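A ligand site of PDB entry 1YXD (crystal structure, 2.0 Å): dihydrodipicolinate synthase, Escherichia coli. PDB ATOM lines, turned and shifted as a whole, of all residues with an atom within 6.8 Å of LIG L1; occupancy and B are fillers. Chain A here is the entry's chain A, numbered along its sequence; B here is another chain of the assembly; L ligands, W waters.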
ATOM      1  N   VAL A  42       3.625   7.577  24.609  1.00  0.00           N
ATOM      2  CA  VAL A  42       4.402   6.541  25.272  1.00  0.00           C
ATOM      3  C   VAL A  42       5.770   6.396  24.584  1.00  0.00           C
ATOM      4  O   VAL A  42       6.154   5.313  24.193  1.00  0.00           O
ATOM      5  CB  VAL A  42       3.637   5.154  25.407  1.00  0.00           C
ATOM      6  CG1 VAL A  42       4.375   4.242  26.369  1.00  0.00           C
ATOM      7  CG2 VAL A  42       2.192   5.344  25.877  1.00  0.00           C
ATOM      8  N   GLU A  47       7.178   7.325  29.886  1.00  0.00           N
ATOM      9  CA  GLU A  47       7.459   6.169  30.735  1.00  0.00           C
ATOM     10  C   GLU A  47       7.186   4.809  30.066  1.00  0.00           C
ATOM     11  O   GLU A  47       6.612   3.901  30.677  1.00  0.00           O
ATOM     12  CB  GLU A  47       6.742   6.297  32.078  1.00  0.00           C
ATOM     13  CG  GLU A  47       7.420   7.313  32.980  1.00  0.00           C
ATOM     14  CD  GLU A  47       6.606   7.666  34.218  1.00  0.00           C
ATOM     15  OE1 GLU A  47       5.804   8.618  34.126  1.00  0.00           O
ATOM     16  OE2 GLU A  47       6.808   7.025  35.291  1.00  0.00           O
ATOM     17  N   SER A  48       7.611   4.691  28.817  1.00  0.00           N
ATOM     18  CA  SER A  48       7.463   3.458  28.063  1.00  0.00           C
ATOM     19  C   SER A  48       8.028   2.264  28.821  1.00  0.00           C
ATOM     20  O   SER A  48       7.439   1.191  28.807  1.00  0.00           O
ATOM     21  CB  SER A  48       8.180   3.576  26.713  1.00  0.00           C
ATOM     22  OG  SER A  48       9.532   3.948  26.927  1.00  0.00           O
ATOM     23  N   ALA A  49       9.173   2.444  29.489  1.00  0.00           N
ATOM     24  CA  ALA A  49       9.839   1.326  30.204  1.00  0.00           C
ATOM     25  C   ALA A  49       8.964   0.631  31.255  1.00  0.00           C
ATOM     26  O   ALA A  49       9.025  -0.582  31.400  1.00  0.00           O
ATOM     27  CB  ALA A  49      11.163   1.813  30.852  1.00  0.00           C
ATOM     28  N   THR A  50       8.187   1.416  32.003  1.00  0.00           N
ATOM     29  CA  THR A  50       7.448   0.911  33.182  1.00  0.00           C
ATOM     30  C   THR A  50       5.966   0.638  32.956  1.00  0.00           C
ATOM     31  O   THR A  50       5.255   0.278  33.906  1.00  0.00           O
ATOM     32  CB  THR A  50       7.610   1.899  34.349  1.00  0.00           C
ATOM     33  OG1 THR A  50       7.264   3.236  33.931  1.00  0.00           O
ATOM     34  CG2 THR A  50       9.089   2.000  34.727  1.00  0.00           C
ATOM     35  N   LEU A  51       5.516   0.804  31.724  1.00  0.00           N
ATOM     36  CA  LEU A  51       4.208   0.336  31.286  1.00  0.00           C
ATOM     37  C   LEU A  51       4.348  -1.009  30.640  1.00  0.00           C
ATOM     38  O   LEU A  51       5.197  -1.165  29.730  1.00  0.00           O
ATOM     39  CB  LEU A  51       3.636   1.319  30.255  1.00  0.00           C
ATOM     40  CG  LEU A  51       2.869   2.545  30.692  1.00  0.00           C
ATOM     41  CD1 LEU A  51       3.219   2.995  32.049  1.00  0.00           C
ATOM     42  CD2 LEU A  51       2.994   3.682  29.656  1.00  0.00           C
ATOM     43  N   ASN A  52       3.523  -1.980  31.041  1.00  0.00           N
ATOM     44  CA  ASN A  52       3.537  -3.247  30.312  1.00  0.00           C
ATOM     45  C   ASN A  52       2.911  -3.067  28.929  1.00  0.00           C
ATOM     46  O   ASN A  52       2.364  -2.008  28.623  1.00  0.00           O
ATOM     47  CB  ASN A  52       2.947  -4.408  31.096  1.00  0.00           C
ATOM     48  CG  ASN A  52       1.444  -4.295  31.278  1.00  0.00           C
ATOM     49  OD1 ASN A  52       0.728  -3.887  30.367  1.00  0.00           O
ATOM     50  ND2 ASN A  52       0.965  -4.689  32.463  1.00  0.00           N
ATOM     51  N   HIS A  53       3.050  -4.082  28.090  1.00  0.00           N
ATOM     52  CA  HIS A  53       2.629  -3.956  26.695  1.00  0.00           C
ATOM     53  C   HIS A  53       1.175  -3.561  26.513  1.00  0.00           C
ATOM     54  O   HIS A  53       0.855  -2.755  25.656  1.00  0.00           O
ATOM     55  CB  HIS A  53       2.910  -5.250  25.911  1.00  0.00           C
ATOM     56  CG  HIS A  53       4.318  -5.334  25.421  1.00  0.00           C
ATOM     57  ND1 HIS A  53       5.349  -5.887  26.149  1.00  0.00           N
ATOM     58  CD2 HIS A  53       4.872  -4.922  24.250  1.00  0.00           C
ATOM     59  CE1 HIS A  53       6.459  -5.812  25.455  1.00  0.00           C
ATOM     60  NE2 HIS A  53       6.207  -5.215  24.304  1.00  0.00           N
ATOM     61  N   ASP A  54       0.300  -4.123  27.332  1.00  0.00           N
ATOM     62  CA  ASP A  54      -1.120  -3.798  27.289  1.00  0.00           C
ATOM     63  C   ASP A  54      -1.402  -2.408  27.786  1.00  0.00           C
ATOM     64  O   ASP A  54      -2.174  -1.677  27.185  1.00  0.00           O
ATOM     65  CB  ASP A  54      -1.903  -4.810  28.111  1.00  0.00           C
ATOM     66  CG  ASP A  54      -1.943  -6.154  27.464  1.00  0.00           C
ATOM     67  OD1 ASP A  54      -2.075  -6.230  26.242  1.00  0.00           O
ATOM     68  OD2 ASP A  54      -1.834  -7.198  28.111  1.00  0.00           O
ATOM     69  N   HIS A  56       0.656   0.100  27.861  1.00  0.00           N
ATOM     70  CA  HIS A  56       1.263   0.946  26.826  1.00  0.00           C
ATOM     71  C   HIS A  56       0.261   1.161  25.677  1.00  0.00           C
ATOM     72  O   HIS A  56      -0.048   2.306  25.287  1.00  0.00           O
ATOM     73  CB  HIS A  56       2.524   0.212  26.348  1.00  0.00           C
ATOM     74  CG  HIS A  56       3.324   0.911  25.289  1.00  0.00           C
ATOM     75  ND1 HIS A  56       4.703   0.815  25.243  1.00  0.00           N
ATOM     76  CD2 HIS A  56       2.964   1.675  24.224  1.00  0.00           C
ATOM     77  CE1 HIS A  56       5.152   1.481  24.180  1.00  0.00           C
ATOM     78  NE2 HIS A  56       4.118   2.014  23.553  1.00  0.00           N
ATOM     79  N   GLY A  78       9.298   1.332  20.149  1.00  0.00           N
ATOM     80  CA  GLY A  78      10.621   0.773  20.263  1.00  0.00           C
ATOM     81  C   GLY A  78      10.697  -0.367  21.262  1.00  0.00           C
ATOM     82  O   GLY A  78       9.880  -0.455  22.191  1.00  0.00           O
ATOM     83  N   ALA A  79      11.648  -1.260  21.030  1.00  0.00           N
ATOM     84  CA  ALA A  79      11.916  -2.397  21.914  1.00  0.00           C
ATOM     85  C   ALA A  79      13.341  -2.891  21.623  1.00  0.00           C
ATOM     86  O   ALA A  79      13.872  -2.676  20.528  1.00  0.00           O
ATOM     87  CB  ALA A  79      10.887  -3.515  21.719  1.00  0.00           C
ATOM     88  N   ASN A  80      13.963  -3.524  22.590  1.00  0.00           N
ATOM     89  CA  ASN A  80      15.312  -4.028  22.348  1.00  0.00           C
ATOM     90  C   ASN A  80      15.358  -5.463  21.838  1.00  0.00           C
ATOM     91  O   ASN A  80      16.442  -5.996  21.620  1.00  0.00           O
ATOM     92  CB  ASN A  80      16.192  -3.824  23.591  1.00  0.00           C
ATOM     93  CG  ASN A  80      15.746  -4.645  24.789  1.00  0.00           C
ATOM     94  OD1 ASN A  80      14.642  -5.212  24.779  1.00  0.00           O
ATOM     95  ND2 ASN A  80      16.596  -4.723  25.825  1.00  0.00           N
ATOM     96  N   ALA A  81      14.176  -6.059  21.694  1.00  0.00           N
ATOM     97  CA  ALA A  81      13.987  -7.338  21.061  1.00  0.00           C
ATOM     98  C   ALA A  81      13.122  -7.087  19.819  1.00  0.00           C
ATOM     99  O   ALA A  81      12.039  -6.475  19.895  1.00  0.00           O
ATOM    100  CB  ALA A  81      13.322  -8.313  22.005  1.00  0.00           C
ATOM    101  N   GLU A  84       9.522  -8.166  19.905  1.00  0.00           N
ATOM    102  CA  GLU A  84       8.674  -7.294  20.722  1.00  0.00           C
ATOM    103  C   GLU A  84       8.272  -6.028  19.987  1.00  0.00           C
ATOM    104  O   GLU A  84       7.146  -5.578  20.095  1.00  0.00           O
ATOM    105  CB  GLU A  84       9.386  -6.855  22.000  1.00  0.00           C
ATOM    106  CG  GLU A  84       9.260  -7.784  23.168  1.00  0.00           C
ATOM    107  CD  GLU A  84       9.916  -7.160  24.392  1.00  0.00           C
ATOM    108  OE1 GLU A  84      11.066  -7.532  24.653  1.00  0.00           O
ATOM    109  OE2 GLU A  84       9.298  -6.260  25.060  1.00  0.00           O
ATOM    110  N   LEU A  88       4.470  -4.876  19.144  1.00  0.00           N
ATOM    111  CA  LEU A  88       3.974  -3.588  19.575  1.00  0.00           C
ATOM    112  C   LEU A  88       3.485  -2.772  18.381  1.00  0.00           C
ATOM    113  O   LEU A  88       2.379  -2.190  18.397  1.00  0.00           O
ATOM    114  CB  LEU A  88       5.068  -2.864  20.356  1.00  0.00           C
ATOM    115  CG  LEU A  88       4.833  -1.715  21.305  1.00  0.00           C
ATOM    116  CD1 LEU A  88       3.641  -1.882  22.242  1.00  0.00           C
ATOM    117  CD2 LEU A  88       6.146  -1.485  22.105  1.00  0.00           C
ATOM    118  N   TYR A 106      18.262  -1.047  23.264  1.00  0.00           N
ATOM    119  CA  TYR A 106      19.016  -0.623  24.447  1.00  0.00           C
ATOM    120  C   TYR A 106      19.484  -1.857  25.210  1.00  0.00           C
ATOM    121  O   TYR A 106      18.886  -2.903  25.123  1.00  0.00           O
ATOM    122  CB  TYR A 106      18.134   0.248  25.331  1.00  0.00           C
ATOM    123  CG  TYR A 106      16.677  -0.211  25.340  1.00  0.00           C
ATOM    124  CD1 TYR A 106      16.219  -1.155  26.279  1.00  0.00           C
ATOM    125  CD2 TYR A 106      15.786   0.277  24.399  1.00  0.00           C
ATOM    126  CE1 TYR A 106      14.885  -1.607  26.263  1.00  0.00           C
ATOM    127  CE2 TYR A 106      14.465  -0.137  24.379  1.00  0.00           C
ATOM    128  CZ  TYR A 106      14.013  -1.084  25.311  1.00  0.00           C
ATOM    129  OH  TYR A 106      12.689  -1.502  25.248  1.00  0.00           O
ATOM    130  N   HIS B  53       9.196 -13.397  29.248  1.00  0.00           N
ATOM    131  CA  HIS B  53       9.242 -13.804  30.654  1.00  0.00           C
ATOM    132  C   HIS B  53       9.080 -15.305  30.858  1.00  0.00           C
ATOM    133  O   HIS B  53       9.764 -15.914  31.676  1.00  0.00           O
ATOM    134  CB  HIS B  53       8.232 -13.009  31.505  1.00  0.00           C
ATOM    135  CG  HIS B  53       8.656 -11.594  31.745  1.00  0.00           C
ATOM    136  ND1 HIS B  53       8.235 -10.540  30.959  1.00  0.00           N
ATOM    137  CD2 HIS B  53       9.487 -11.069  32.664  1.00  0.00           C
ATOM    138  CE1 HIS B  53       8.784  -9.424  31.399  1.00  0.00           C
ATOM    139  NE2 HIS B  53       9.558  -9.710  32.431  1.00  0.00           N
ATOM    140  N   ALA B  79      15.517  -6.008  35.590  1.00  0.00           N
ATOM    141  CA  ALA B  79      14.509  -5.338  34.750  1.00  0.00           C
ATOM    142  C   ALA B  79      14.645  -3.836  34.933  1.00  0.00           C
ATOM    143  O   ALA B  79      15.164  -3.377  35.976  1.00  0.00           O
ATOM    144  CB  ALA B  79      13.069  -5.817  35.093  1.00  0.00           C
ATOM    145  N   ASN B  80      14.195  -3.062  33.954  1.00  0.00           N
ATOM    146  CA  ASN B  80      14.238  -1.599  34.077  1.00  0.00           C
ATOM    147  C   ASN B  80      12.966  -1.015  34.690  1.00  0.00           C
ATOM    148  O   ASN B  80      12.851   0.197  34.826  1.00  0.00           O
ATOM    149  CB  ASN B  80      14.597  -0.899  32.761  1.00  0.00           C
ATOM    150  CG  ASN B  80      13.631  -1.172  31.666  1.00  0.00           C
ATOM    151  OD1 ASN B  80      12.777  -2.037  31.783  1.00  0.00           O
ATOM    152  ND2 ASN B  80      13.783  -0.462  30.530  1.00  0.00           N
ATOM    153  N   ALA B  81      12.018  -1.898  35.008  1.00  0.00           N
ATOM    154  CA  ALA B  81      10.806  -1.516  35.727  1.00  0.00           C
ATOM    155  C   ALA B  81      10.804  -2.328  37.003  1.00  0.00           C
ATOM    156  O   ALA B  81      10.937  -3.546  36.965  1.00  0.00           O
ATOM    157  CB  ALA B  81       9.570  -1.856  34.874  1.00  0.00           C
ATOM    158  N   GLU B  84       8.433  -5.364  37.121  1.00  0.00           N
ATOM    159  CA  GLU B  84       8.897  -6.487  36.350  1.00  0.00           C
ATOM    160  C   GLU B  84       9.970  -7.279  37.089  1.00  0.00           C
ATOM    161  O   GLU B  84       9.997  -8.515  37.025  1.00  0.00           O
ATOM    162  CB  GLU B  84       9.485  -6.065  35.012  1.00  0.00           C
ATOM    163  CG  GLU B  84       8.526  -5.506  34.014  1.00  0.00           C
ATOM    164  CD  GLU B  84       9.246  -5.159  32.707  1.00  0.00           C
ATOM    165  OE1 GLU B  84       9.794  -6.087  32.048  1.00  0.00           O
ATOM    166  OE2 GLU B  84       9.299  -3.979  32.356  1.00  0.00           O
ATOM    167  N   TYR B 106      18.014  -0.040  32.887  1.00  0.00           N
ATOM    168  CA  TYR B 106      18.598   0.445  31.615  1.00  0.00           C
ATOM    169  C   TYR B 106      17.581   1.289  30.859  1.00  0.00           C
ATOM    170  O   TYR B 106      16.376   1.124  31.035  1.00  0.00           O
ATOM    171  CB  TYR B 106      19.031  -0.725  30.715  1.00  0.00           C
ATOM    172  CG  TYR B 106      18.121  -1.912  30.837  1.00  0.00           C
ATOM    173  CD1 TYR B 106      17.032  -2.058  29.997  1.00  0.00           C
ATOM    174  CD2 TYR B 106      18.341  -2.881  31.816  1.00  0.00           C
ATOM    175  CE1 TYR B 106      16.179  -3.149  30.113  1.00  0.00           C
ATOM    176  CE2 TYR B 106      17.505  -3.988  31.939  1.00  0.00           C
ATOM    177  CZ  TYR B 106      16.412  -4.102  31.083  1.00  0.00           C
ATOM    178  OH  TYR B 106      15.589  -5.193  31.196  1.00  0.00           O
ATOM    179  N   TYR B 107      18.106   2.249  30.077  1.00  0.00           N
ATOM    180  CA  TYR B 107      17.331   3.131  29.206  1.00  0.00           C
ATOM    181  C   TYR B 107      16.673   4.329  29.922  1.00  0.00           C
ATOM    182  O   TYR B 107      16.802   5.482  29.482  1.00  0.00           O
ATOM    183  CB  TYR B 107      16.292   2.331  28.407  1.00  0.00           C
ATOM    184  CG  TYR B 107      15.565   3.156  27.381  1.00  0.00           C
ATOM    185  CD1 TYR B 107      16.224   3.621  26.261  1.00  0.00           C
ATOM    186  CD2 TYR B 107      14.246   3.525  27.568  1.00  0.00           C
ATOM    187  CE1 TYR B 107      15.579   4.394  25.311  1.00  0.00           C
ATOM    188  CE2 TYR B 107      13.584   4.334  26.602  1.00  0.00           C
ATOM    189  CZ  TYR B 107      14.271   4.755  25.470  1.00  0.00           C
ATOM    190  OH  TYR B 107      13.649   5.550  24.502  1.00  0.00           O
HETATM  191  N1  LIG L   1      10.429  -2.751  30.533  1.00  0.00           N
HETATM  192  C1  LIG L   1      10.633  -3.398  29.199  1.00  0.00           C
HETATM  193  C2  LIG L   1      11.455  -2.517  28.300  1.00  0.00           C
HETATM  194  O1  LIG L   1      11.708  -1.351  28.625  1.00  0.00           O
HETATM  195  C3  LIG L   1       9.309  -3.711  28.493  1.00  0.00           C
HETATM  196  C4  LIG L   1       8.484  -2.491  28.067  1.00  0.00           C
HETATM  197  C5  LIG L   1       7.100  -2.957  27.593  1.00  0.00           C
HETATM  198  C6  LIG L   1       6.366  -2.035  26.644  1.00  0.00           C
HETATM  199  N2  LIG L   1       6.293  -0.675  27.163  1.00  0.00           N
HETATM  200  O2  LIG L   1      11.897  -2.940  27.234  1.00  0.00           O
HETATM  201  N1  LG2 L   2      13.156  -6.941  26.163  1.00  0.00           N
HETATM  202  C1  LG2 L   2      12.727  -6.499  27.518  1.00  0.00           C
HETATM  203  C2  LG2 L   2      13.929  -6.100  28.319  1.00  0.00           C
HETATM  204  O1  LG2 L   2      13.776  -5.551  29.422  1.00  0.00           O
HETATM  205  C3  LG2 L   2      11.871  -7.558  28.258  1.00  0.00           C
HETATM  206  C4  LG2 L   2      12.667  -8.752  28.813  1.00  0.00           C
HETATM  207  C5  LG2 L   2      11.765  -9.904  29.173  1.00  0.00           C
HETATM  208  C6  LG2 L   2      12.376 -10.860  30.184  1.00  0.00           C
HETATM  209  N2  LG2 L   2      13.687 -11.388  29.798  1.00  0.00           N
HETATM  210  O2  LG2 L   2      15.081  -6.290  27.866  1.00  0.00           O
HETATM  211  O   HOH W   1      11.147   1.013  26.730  1.00  0.00           O
HETATM  212  O   HOH W   2      10.851  -4.182  25.114  1.00  0.00           O
HETATM  213  O   HOH W   3       8.750   0.163  25.809  1.00  0.00           O
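The side-chain carboxylate (OE2) of Glu 84 of chain B is in salt-bridge range of a nitrogen (N1) of LIG L1 (2.5 Å). OH of Tyr 106 of chain A sits at hydrogen-bond distance from O2 of LIG L1 (2.6 Å). O of Ala 49 is in hydrogen-bond range of N1 of LIG L1 (2.7 Å). The backbone carbonyl oxygen (O) of Ser 48 sits at hydrogen-bond distance from a nitrogen (N2) of LIG L1, 2.7 Å away. A nitrogen (N1) of LIG L1 is in hydrogen-bond range of the side-chain amide oxygen (OD1) of Asn 80 of chain B, 2.8 Å away. N2 of LIG L1 lies within hydrogen-bond range of O of Leu 51 (2.8 Å). A ring nitrogen (ND1) of His 56 sits at hydrogen-bond distance from a nitrogen (N2) of LIG L1, 2.9 Å away. OE1 of Glu 84 of chain A lies within salt-bridge range of N1 of LG2 L2, at 2.6 Å. The side-chain amide oxygen (OD1) of Asn 80 of chain A sits at hydrogen-bond distance from a nitrogen (N1) of LG2 L2 (2.7 Å). OH of Tyr 106 of chain B sits at hydrogen-bond distance from O1 of LG2 L2, 2.6 Å away.
The backbone carbonyl oxygen (O) of Tyr 106 of chain A lies within hydrogen-bond range of the side-chain amide nitrogen (ND2) of Asn 80 of chain A, 3.0 Å away. O of Tyr 106 of chain B is in hydrogen-bond range of ND2 of Asn 80 of chain B, at 3.1 Å. The side-chain carboxylate of Glu 84 of chain A lies close to a ring nitrogen (NE2) of His 53 of chain A (3.3 Å).
CE1 of His 53 of chain A touches C5 of LIG L1 (3.6 Å). Hydrophobic or aromatic side chains that line LIG L1: Ala 49, His 53 of chain A, His 56 and Tyr 106 of chain A. Eight residues have an atom within 4 Å of LIG L1: Ser 48, Ala 49, Leu 51, His 53 of chain A, His 56, Tyr 106 of chain A, Asn 80 of chain B and Glu 84 of chain B.
Water W2 lies within hydrogen-bond range of OE2 of Glu 84 of chain A (2.6 Å), O2 of LIG L1 (2.7 Å) and OH of Tyr 106 of chain A (3.3 Å). Water W3 lies within hydrogen-bond range of a nitrogen (N2) of LIG L1 (2.9 Å) and the backbone carbonyl oxygen of Ser 48 (3.4 Å). Water W1 lies within hydrogen-bond range of an oxygen (O1) of LIG L1 (3.1 Å), the side-chain hydroxyl of Tyr 106 of chain A (3.3 Å) and the side-chain hydroxyl of Ser 48 (3.4 Å).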
